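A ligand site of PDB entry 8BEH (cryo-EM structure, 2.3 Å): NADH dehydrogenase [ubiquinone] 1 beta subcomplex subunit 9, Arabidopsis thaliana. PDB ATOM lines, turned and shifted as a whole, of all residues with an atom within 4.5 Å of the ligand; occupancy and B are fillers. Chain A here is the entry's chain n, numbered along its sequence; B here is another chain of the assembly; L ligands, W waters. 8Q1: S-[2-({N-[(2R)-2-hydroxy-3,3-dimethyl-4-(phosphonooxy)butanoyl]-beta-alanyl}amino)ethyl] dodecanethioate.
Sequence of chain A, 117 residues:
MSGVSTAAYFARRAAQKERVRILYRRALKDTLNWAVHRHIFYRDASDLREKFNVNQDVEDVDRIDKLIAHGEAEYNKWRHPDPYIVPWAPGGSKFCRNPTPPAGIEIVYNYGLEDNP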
ATOM      1  N   ARG A  13      32.145  36.715 -12.169  1.00  0.00           N
ATOM      2  CA  ARG A  13      31.203  36.294 -11.113  1.00  0.00           C
ATOM      3  C   ARG A  13      30.228  35.286 -11.745  1.00  0.00           C
ATOM      4  O   ARG A  13      29.924  34.260 -11.091  1.00  0.00           O
ATOM      5  CB  ARG A  13      30.574  37.539 -10.454  1.00  0.00           C
ATOM      6  CG  ARG A  13      31.499  38.246  -9.471  1.00  0.00           C
ATOM      7  CD  ARG A  13      31.548  37.653  -8.079  1.00  0.00           C
ATOM      8  NE  ARG A  13      30.240  37.330  -7.543  1.00  0.00           N
ATOM      9  CZ  ARG A  13      29.785  36.096  -7.402  1.00  0.00           C
ATOM     10  NH1 ARG A  13      30.527  35.075  -7.771  1.00  0.00           N
ATOM     11  NH2 ARG A  13      28.586  35.897  -6.890  1.00  0.00           N
ATOM     12  N   LYS A  17      29.461  31.354 -10.682  1.00  0.00           N
ATOM     13  CA  LYS A  17      28.100  30.857 -10.476  1.00  0.00           C
ATOM     14  C   LYS A  17      27.925  29.510 -11.180  1.00  0.00           C
ATOM     15  O   LYS A  17      27.381  28.626 -10.553  1.00  0.00           O
ATOM     16  CB  LYS A  17      27.156  31.947 -10.924  1.00  0.00           C
ATOM     17  CG  LYS A  17      26.980  33.116  -9.974  1.00  0.00           C
ATOM     18  CD  LYS A  17      25.898  34.054 -10.441  1.00  0.00           C
ATOM     19  CE  LYS A  17      25.870  35.355  -9.683  1.00  0.00           C
ATOM     20  NZ  LYS A  17      27.238  35.875  -9.466  1.00  0.00           N
ATOM     21  N   VAL A  20      29.557  26.745  -9.199  1.00  0.00           N
ATOM     22  CA  VAL A  20      28.779  26.380  -8.005  1.00  0.00           C
ATOM     23  C   VAL A  20      27.524  25.565  -8.410  1.00  0.00           C
ATOM     24  O   VAL A  20      27.369  24.501  -7.860  1.00  0.00           O
ATOM     25  CB  VAL A  20      28.479  27.559  -7.066  1.00  0.00           C
ATOM     26  CG1 VAL A  20      27.631  27.162  -5.861  1.00  0.00           C
ATOM     27  CG2 VAL A  20      29.740  28.276  -6.639  1.00  0.00           C
ATOM     28  N   ARG A  21      26.779  25.997  -9.422  1.00  0.00           N
ATOM     29  CA  ARG A  21      25.560  25.284  -9.903  1.00  0.00           C
ATOM     30  C   ARG A  21      25.889  23.874 -10.417  1.00  0.00           C
ATOM     31  O   ARG A  21      25.084  22.985 -10.207  1.00  0.00           O
ATOM     32  CB  ARG A  21      24.782  26.152 -10.888  1.00  0.00           C
ATOM     33  CG  ARG A  21      24.060  27.329 -10.252  1.00  0.00           C
ATOM     34  CD  ARG A  21      23.061  27.944 -11.201  1.00  0.00           C
ATOM     35  NE  ARG A  21      23.661  28.127 -12.502  1.00  0.00           N
ATOM     36  CZ  ARG A  21      24.266  29.223 -12.925  1.00  0.00           C
ATOM     37  NH1 ARG A  21      24.322  30.291 -12.159  1.00  0.00           N
ATOM     38  NH2 ARG A  21      24.813  29.229 -14.119  1.00  0.00           N
ATOM     39  N   LEU A  23      28.655  22.102  -9.486  1.00  0.00           N
ATOM     40  CA  LEU A  23      29.153  21.371  -8.296  1.00  0.00           C
ATOM     41  C   LEU A  23      27.938  20.847  -7.504  1.00  0.00           C
ATOM     42  O   LEU A  23      27.938  19.640  -7.153  1.00  0.00           O
ATOM     43  CB  LEU A  23      30.040  22.248  -7.408  1.00  0.00           C
ATOM     44  CG  LEU A  23      30.458  21.643  -6.071  1.00  0.00           C
ATOM     45  CD1 LEU A  23      31.359  20.442  -6.260  1.00  0.00           C
ATOM     46  CD2 LEU A  23      31.094  22.668  -5.169  1.00  0.00           C
ATOM     47  N   ALA A  27      27.044  16.868  -6.706  1.00  0.00           N
ATOM     48  CA  ALA A  27      26.990  16.465  -5.272  1.00  0.00           C
ATOM     49  C   ALA A  27      25.622  15.857  -4.987  1.00  0.00           C
ATOM     50  O   ALA A  27      25.603  14.760  -4.449  1.00  0.00           O
ATOM     51  CB  ALA A  27      27.350  17.621  -4.333  1.00  0.00           C
ATOM     52  N   ASP A  30      25.226  12.367  -6.569  1.00  0.00           N
ATOM     53  CA  ASP A  30      26.047  11.419  -5.832  1.00  0.00           C
ATOM     54  C   ASP A  30      25.433  11.096  -4.460  1.00  0.00           C
ATOM     55  O   ASP A  30      25.691  10.028  -3.996  1.00  0.00           O
ATOM     56  CB  ASP A  30      27.471  11.942  -5.728  1.00  0.00           C
ATOM     57  CG  ASP A  30      28.496  10.836  -5.673  1.00  0.00           C
ATOM     58  OD1 ASP A  30      28.632  10.124  -6.678  1.00  0.00           O
ATOM     59  OD2 ASP A  30      29.134  10.696  -4.618  1.00  0.00           O
ATOM     60  N   LEU A  48      23.053  18.617   2.323  1.00  0.00           N
ATOM     61  CA  LEU A  48      23.976  19.175   1.303  1.00  0.00           C
ATOM     62  C   LEU A  48      23.556  20.597   0.916  1.00  0.00           C
ATOM     63  O   LEU A  48      24.453  21.578   0.807  1.00  0.00           O
ATOM     64  CB  LEU A  48      24.023  18.210   0.121  1.00  0.00           C
ATOM     65  CG  LEU A  48      24.807  18.654  -1.096  1.00  0.00           C
ATOM     66  CD1 LEU A  48      26.289  18.376  -0.916  1.00  0.00           C
ATOM     67  CD2 LEU A  48      24.271  17.967  -2.333  1.00  0.00           C
ATOM     68  N   LYS A  51      24.850  22.992   3.551  1.00  0.00           N
ATOM     69  CA  LYS A  51      26.249  23.434   3.288  1.00  0.00           C
ATOM     70  C   LYS A  51      26.296  24.624   2.255  1.00  0.00           C
ATOM     71  O   LYS A  51      26.779  25.930   2.531  1.00  0.00           O
ATOM     72  CB  LYS A  51      27.035  22.189   2.869  1.00  0.00           C
ATOM     73  CG  LYS A  51      27.129  21.063   3.882  1.00  0.00           C
ATOM     74  CD  LYS A  51      28.001  19.939   3.381  1.00  0.00           C
ATOM     75  CE  LYS A  51      27.922  18.706   4.243  1.00  0.00           C
ATOM     76  NZ  LYS A  51      29.045  17.776   4.001  1.00  0.00           N
ATOM     77  N   PHE A  52      25.657  24.382   1.116  1.00  0.00           N
ATOM     78  CA  PHE A  52      25.754  25.526   0.155  1.00  0.00           C
ATOM     79  C   PHE A  52      25.060  26.777   0.740  1.00  0.00           C
ATOM     80  O   PHE A  52      25.535  27.878   0.585  1.00  0.00           O
ATOM     81  CB  PHE A  52      25.246  25.172  -1.232  1.00  0.00           C
ATOM     82  CG  PHE A  52      26.044  24.170  -2.012  1.00  0.00           C
ATOM     83  CD1 PHE A  52      26.074  22.828  -1.654  1.00  0.00           C
ATOM     84  CD2 PHE A  52      26.754  24.547  -3.145  1.00  0.00           C
ATOM     85  CE1 PHE A  52      26.788  21.901  -2.382  1.00  0.00           C
ATOM     86  CE2 PHE A  52      27.482  23.622  -3.871  1.00  0.00           C
ATOM     87  CZ  PHE A  52      27.496  22.295  -3.491  1.00  0.00           C
ATOM     88  N   ASN A  55      27.190  29.109   2.974  1.00  0.00           N
ATOM     89  CA  ASN A  55      28.033  30.141   2.251  1.00  0.00           C
ATOM     90  C   ASN A  55      27.319  30.954   1.161  1.00  0.00           C
ATOM     91  O   ASN A  55      28.023  31.751   0.516  1.00  0.00           O
ATOM     92  CB  ASN A  55      29.259  29.579   1.547  1.00  0.00           C
ATOM     93  CG  ASN A  55      30.165  28.789   2.460  1.00  0.00           C
ATOM     94  OD1 ASN A  55      30.075  27.571   2.509  1.00  0.00           O
ATOM     95  ND2 ASN A  55      31.042  29.476   3.159  1.00  0.00           N
ATOM     96  N   GLN A  56      26.013  30.809   0.934  1.00  0.00           N
ATOM     97  CA  GLN A  56      25.296  31.486  -0.227  1.00  0.00           C
ATOM     98  C   GLN A  56      25.486  32.996  -0.266  1.00  0.00           C
ATOM     99  O   GLN A  56      25.278  33.632  -1.304  1.00  0.00           O
ATOM    100  CB  GLN A  56      23.771  31.308  -0.161  1.00  0.00           C
ATOM    101  CG  GLN A  56      23.055  31.995   0.974  1.00  0.00           C
ATOM    102  CD  GLN A  56      21.619  31.541   1.091  1.00  0.00           C
ATOM    103  OE1 GLN A  56      21.294  30.369   0.916  1.00  0.00           O
ATOM    104  NE2 GLN A  56      20.746  32.487   1.386  1.00  0.00           N
ATOM    105  N   VAL A  58      28.184  34.930   0.680  1.00  0.00           N
ATOM    106  CA  VAL A  58      29.519  35.557   0.580  1.00  0.00           C
ATOM    107  C   VAL A  58      29.631  36.473  -0.647  1.00  0.00           C
ATOM    108  O   VAL A  58      29.095  36.157  -1.697  1.00  0.00           O
ATOM    109  CB  VAL A  58      30.608  34.459   0.670  1.00  0.00           C
ATOM    110  CG1 VAL A  58      31.982  34.941   0.234  1.00  0.00           C
ATOM    111  CG2 VAL A  58      30.635  33.721   1.984  1.00  0.00           C
ATOM    112  N   ILE A  64      35.398  33.179  -2.739  1.00  0.00           N
ATOM    113  CA  ILE A  64      34.475  32.328  -3.525  1.00  0.00           C
ATOM    114  C   ILE A  64      35.348  31.330  -4.279  1.00  0.00           C
ATOM    115  O   ILE A  64      35.026  30.143  -4.238  1.00  0.00           O
ATOM    116  CB  ILE A  64      33.482  33.098  -4.429  1.00  0.00           C
ATOM    117  CG1 ILE A  64      32.450  33.899  -3.634  1.00  0.00           C
ATOM    118  CG2 ILE A  64      32.823  32.175  -5.438  1.00  0.00           C
ATOM    119  CD1 ILE A  64      31.835  35.021  -4.438  1.00  0.00           C
ATOM    120  N   LEU A  67      36.576  28.620  -1.940  1.00  0.00           N
ATOM    121  CA  LEU A  67      35.460  27.710  -1.587  1.00  0.00           C
ATOM    122  C   LEU A  67      35.097  26.801  -2.765  1.00  0.00           C
ATOM    123  O   LEU A  67      34.755  25.667  -2.549  1.00  0.00           O
ATOM    124  CB  LEU A  67      34.261  28.528  -1.093  1.00  0.00           C
ATOM    125  CG  LEU A  67      34.443  29.304   0.197  1.00  0.00           C
ATOM    126  CD1 LEU A  67      33.240  30.191   0.497  1.00  0.00           C
ATOM    127  CD2 LEU A  67      34.721  28.370   1.351  1.00  0.00           C
ATOM    128  N   ILE A  68      35.111  27.340  -3.979  1.00  0.00           N
ATOM    129  CA  ILE A  68      34.794  26.500  -5.122  1.00  0.00           C
ATOM    130  C   ILE A  68      35.831  25.396  -5.273  1.00  0.00           C
ATOM    131  O   ILE A  68      35.500  24.232  -5.457  1.00  0.00           O
ATOM    132  CB  ILE A  68      34.677  27.339  -6.411  1.00  0.00           C
ATOM    133  CG1 ILE A  68      33.430  28.213  -6.383  1.00  0.00           C
ATOM    134  CG2 ILE A  68      34.638  26.442  -7.626  1.00  0.00           C
ATOM    135  CD1 ILE A  68      33.443  29.279  -7.460  1.00  0.00           C
ATOM    136  N   GLY A  71      35.338  22.811  -2.579  1.00  0.00           N
ATOM    137  CA  GLY A  71      34.142  22.003  -2.866  1.00  0.00           C
ATOM    138  C   GLY A  71      34.386  20.995  -3.977  1.00  0.00           C
ATOM    139  O   GLY A  71      34.043  19.808  -3.752  1.00  0.00           O
ATOM    140  N   GLU A  74      36.545  18.220  -2.530  1.00  0.00           N
ATOM    141  CA  GLU A  74      35.688  17.373  -1.665  1.00  0.00           C
ATOM    142  C   GLU A  74      34.865  16.415  -2.517  1.00  0.00           C
ATOM    143  O   GLU A  74      35.076  15.222  -2.319  1.00  0.00           O
ATOM    144  CB  GLU A  74      34.951  18.335  -0.746  1.00  0.00           C
ATOM    145  CG  GLU A  74      35.864  19.075   0.201  1.00  0.00           C
ATOM    146  CD  GLU A  74      36.706  18.190   1.112  1.00  0.00           C
ATOM    147  OE1 GLU A  74      36.172  17.186   1.601  1.00  0.00           O
ATOM    148  OE2 GLU A  74      37.900  18.525   1.328  1.00  0.00           O
ATOM    149  N   TYR A  75      34.121  16.900  -3.538  1.00  0.00           N
ATOM    150  CA  TYR A  75      33.409  16.028  -4.484  1.00  0.00           C
ATOM    151  C   TYR A  75      34.346  14.962  -5.022  1.00  0.00           C
ATOM    152  O   TYR A  75      34.058  13.781  -4.847  1.00  0.00           O
ATOM    153  CB  TYR A  75      32.764  16.755  -5.673  1.00  0.00           C
ATOM    154  CG  TYR A  75      32.135  15.891  -6.726  1.00  0.00           C
ATOM    155  CD1 TYR A  75      30.898  15.310  -6.514  1.00  0.00           C
ATOM    156  CD2 TYR A  75      32.770  15.669  -7.932  1.00  0.00           C
ATOM    157  CE1 TYR A  75      30.317  14.505  -7.472  1.00  0.00           C
ATOM    158  CE2 TYR A  75      32.204  14.868  -8.896  1.00  0.00           C
ATOM    159  CZ  TYR A  75      30.965  14.285  -8.674  1.00  0.00           C
ATOM    160  OH  TYR A  75      30.410  13.501  -9.633  1.00  0.00           O
ATOM    161  N   TRP A  78      35.163  12.271  -2.175  1.00  0.00           N
ATOM    162  CA  TRP A  78      34.067  11.464  -1.547  1.00  0.00           C
ATOM    163  C   TRP A  78      33.108  10.949  -2.621  1.00  0.00           C
ATOM    164  O   TRP A  78      32.062  10.393  -2.271  1.00  0.00           O
ATOM    165  CB  TRP A  78      33.403  12.298  -0.432  1.00  0.00           C
ATOM    166  CG  TRP A  78      34.311  12.739   0.667  1.00  0.00           C
ATOM    167  CD1 TRP A  78      34.742  14.003   0.914  1.00  0.00           C
ATOM    168  CD2 TRP A  78      34.908  11.909   1.667  1.00  0.00           C
ATOM    169  NE1 TRP A  78      35.566  14.014   2.007  1.00  0.00           N
ATOM    170  CE2 TRP A  78      35.682  12.757   2.495  1.00  0.00           C
ATOM    171  CE3 TRP A  78      34.867  10.548   1.966  1.00  0.00           C
ATOM    172  CZ2 TRP A  78      36.397  12.288   3.598  1.00  0.00           C
ATOM    173  CZ3 TRP A  78      35.572  10.080   3.046  1.00  0.00           C
ATOM    174  CH2 TRP A  78      36.330  10.938   3.842  1.00  0.00           C
ATOM    175  N   GLN B  72      13.861  32.239 -11.935  1.00  0.00           N
ATOM    176  CA  GLN B  72      14.461  33.265 -11.039  1.00  0.00           C
ATOM    177  C   GLN B  72      13.879  34.632 -11.356  1.00  0.00           C
ATOM    178  O   GLN B  72      14.434  35.612 -10.886  1.00  0.00           O
ATOM    179  CB  GLN B  72      15.987  33.279 -11.173  1.00  0.00           C
ATOM    180  CG  GLN B  72      16.744  32.099 -10.614  1.00  0.00           C
ATOM    181  CD  GLN B  72      18.140  32.513 -10.216  1.00  0.00           C
ATOM    182  OE1 GLN B  72      19.096  32.334 -10.973  1.00  0.00           O
ATOM    183  NE2 GLN B  72      18.274  33.084  -9.033  1.00  0.00           N
ATOM    184  N   ASP B  78      15.870  30.802  -6.066  1.00  0.00           N
ATOM    185  CA  ASP B  78      17.311  30.790  -6.284  1.00  0.00           C
ATOM    186  C   ASP B  78      17.665  29.736  -7.331  1.00  0.00           C
ATOM    187  O   ASP B  78      16.860  28.860  -7.661  1.00  0.00           O
ATOM    188  CB  ASP B  78      18.029  30.520  -4.971  1.00  0.00           C
ATOM    189  CG  ASP B  78      17.426  31.269  -3.801  1.00  0.00           C
ATOM    190  OD1 ASP B  78      16.781  32.315  -4.043  1.00  0.00           O
ATOM    191  OD2 ASP B  78      17.600  30.825  -2.643  1.00  0.00           O
ATOM    192  N   SER B  79      18.815  29.946  -7.923  1.00  0.00           N
ATOM    193  CA  SER B  79      19.311  29.029  -8.984  1.00  0.00           C
ATOM    194  C   SER B  79      19.698  27.620  -8.465  1.00  0.00           C
ATOM    195  O   SER B  79      19.759  26.771  -9.327  1.00  0.00           O
ATOM    196  CB  SER B  79      20.374  29.688  -9.735  1.00  0.00           C
ATOM    197  OG  SER B  79      21.610  29.453  -9.105  1.00  0.00           O
HETATM  198  O4  8Q1 L   1      30.559  27.210  -0.695  1.00  0.00           O
HETATM  199  C16 8Q1 L   1      30.139  13.796  -2.137  1.00  0.00           C
HETATM  200  O3  8Q1 L   1      21.356  31.745  -8.080  1.00  0.00           O
HETATM  201  C15 8Q1 L   1      30.491  15.198  -2.532  1.00  0.00           C
HETATM  202  C14 8Q1 L   1      30.961  16.049  -1.388  1.00  0.00           C
HETATM  203  C13 8Q1 L   1      30.089  17.245  -1.132  1.00  0.00           C
HETATM  204  O2  8Q1 L   1      22.810  31.495 -10.110  1.00  0.00           O
HETATM  205  C12 8Q1 L   1      30.606  18.519  -1.721  1.00  0.00           C
HETATM  206  C11 8Q1 L   1      30.566  19.691  -0.784  1.00  0.00           C
HETATM  207  C10 8Q1 L   1      30.546  21.022  -1.488  1.00  0.00           C
HETATM  208  C9  8Q1 L   1      30.803  22.200  -0.595  1.00  0.00           C
HETATM  209  C8  8Q1 L   1      29.567  22.970  -0.254  1.00  0.00           C
HETATM  210  C7  8Q1 L   1      29.720  24.477  -0.322  1.00  0.00           C
HETATM  211  C6  8Q1 L   1      30.436  24.964  -1.534  1.00  0.00           C
HETATM  212  C1  8Q1 L   1      30.502  26.467  -1.640  1.00  0.00           C
HETATM  213  C28 8Q1 L   1      23.627  30.876  -6.518  1.00  0.00           C
HETATM  214  C29 8Q1 L   1      24.916  31.176  -5.770  1.00  0.00           C
HETATM  215  C30 8Q1 L   1      24.889  30.543  -4.371  1.00  0.00           C
HETATM  216  C31 8Q1 L   1      26.091  30.587  -6.553  1.00  0.00           C
HETATM  217  C32 8Q1 L   1      25.019  32.713  -5.654  1.00  0.00           C
HETATM  218  C34 8Q1 L   1      26.418  33.329  -5.733  1.00  0.00           C
HETATM  219  C37 8Q1 L   1      27.275  33.106  -3.423  1.00  0.00           C
HETATM  220  C38 8Q1 L   1      28.744  32.974  -3.172  1.00  0.00           C
HETATM  221  C39 8Q1 L   1      29.120  31.629  -3.746  1.00  0.00           C
HETATM  222  C42 8Q1 L   1      29.658  29.635  -2.334  1.00  0.00           C
HETATM  223  C43 8Q1 L   1      30.567  28.820  -3.250  1.00  0.00           C
HETATM  224  N36 8Q1 L   1      26.959  33.835  -4.629  1.00  0.00           N
HETATM  225  N41 8Q1 L   1      28.763  30.546  -3.042  1.00  0.00           N
HETATM  226  O27 8Q1 L   1      23.813  31.264  -7.908  1.00  0.00           O
HETATM  227  O33 8Q1 L   1      24.393  33.109  -4.461  1.00  0.00           O
HETATM  228  O35 8Q1 L   1      26.952  33.467  -6.817  1.00  0.00           O
HETATM  229  O40 8Q1 L   1      29.646  31.557  -4.856  1.00  0.00           O
HETATM  230  P24 8Q1 L   1      22.662  32.057  -8.723  1.00  0.00           P
HETATM  231  S44 8Q1 L   1      30.501  27.003  -3.317  1.00  0.00           S
HETATM  232  O1  8Q1 L   1      22.954  33.548  -8.652  1.00  0.00           O
HETATM  233  O   HOH W   1      29.268  32.646  -7.226  1.00  0.00           O
HETATM  234  O   HOH W   2      21.337  32.654  -5.790  1.00  0.00           O
HETATM  235  O   HOH W   3      20.764  29.472  -5.702  1.00  0.00           O
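O4 of the ligand sits close to OD1 of Asn 55, 3.3 Å away. O35 of the ligand lies within hydrogen-bond range of NH2 of Arg 13 (2.9 Å). The backbone carbonyl oxygen (O) of Gln 56 sits close to an oxygen (O33) of the ligand (3.3 Å). The side-chain amide nitrogen of Gln 72 of chain B is in hydrogen-bond range of an oxygen (O3) of the ligand (3.5 Å). NH1 of Arg 21 is in salt-bridge range of O2 of the ligand. OG of Ser 79 of chain B is in hydrogen-bond range of O3 of the ligand (2.5 Å). An oxygen (O3) of the ligand sits close to the backbone NH of Ser 79 of chain B, at 3.1 Å.
Water W1 lies within hydrogen-bond range of O35 of the ligand (2.5 Å) and NH1 of Arg 13 (2.8 Å). Water W3 lies within hydrogen-bond range of N of Ser 79 of chain B (3.0 Å) and O3 of the ligand (3.3 Å).
Lys 17 touches the ligand (CG to O35, 3.2 Å). CG2 of Val 20 touches C43 of the ligand, at 3.5 Å. Leu 48 touches the ligand. Phe 52 touches the ligand (CE1 to C8, 3.7 Å). O of Val 58 touches C38 of the ligand (3.5 Å). Ile 64 touches the ligand. CB of Leu 67 touches O4 of the ligand, 3.9 Å away. CA of Gly 71 touches C10 of the ligand, 3.97 Å away. CA of Tyr 75 touches C15 of the ligand, 3.6 Å away. O of Trp 78 of chain A touches C16 of the ligand, at 3.9 Å. Hydrophobic or aromatic side chains that line the ligand: Val 20, Leu 48, Phe 52, Ile 64, Leu 67 and Trp 78 of chain A.
The indole nitrogen (NE1) of Trp 78 of chain A lies within hydrogen-bond range of the side-chain carboxylate (OE1) of Glu 74 (3.3 Å). The backbone NH (N) of Ser 79 of chain B lies close to the side-chain amide nitrogen (NE2) of Gln 72 of chain B, 3.4 Å away.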
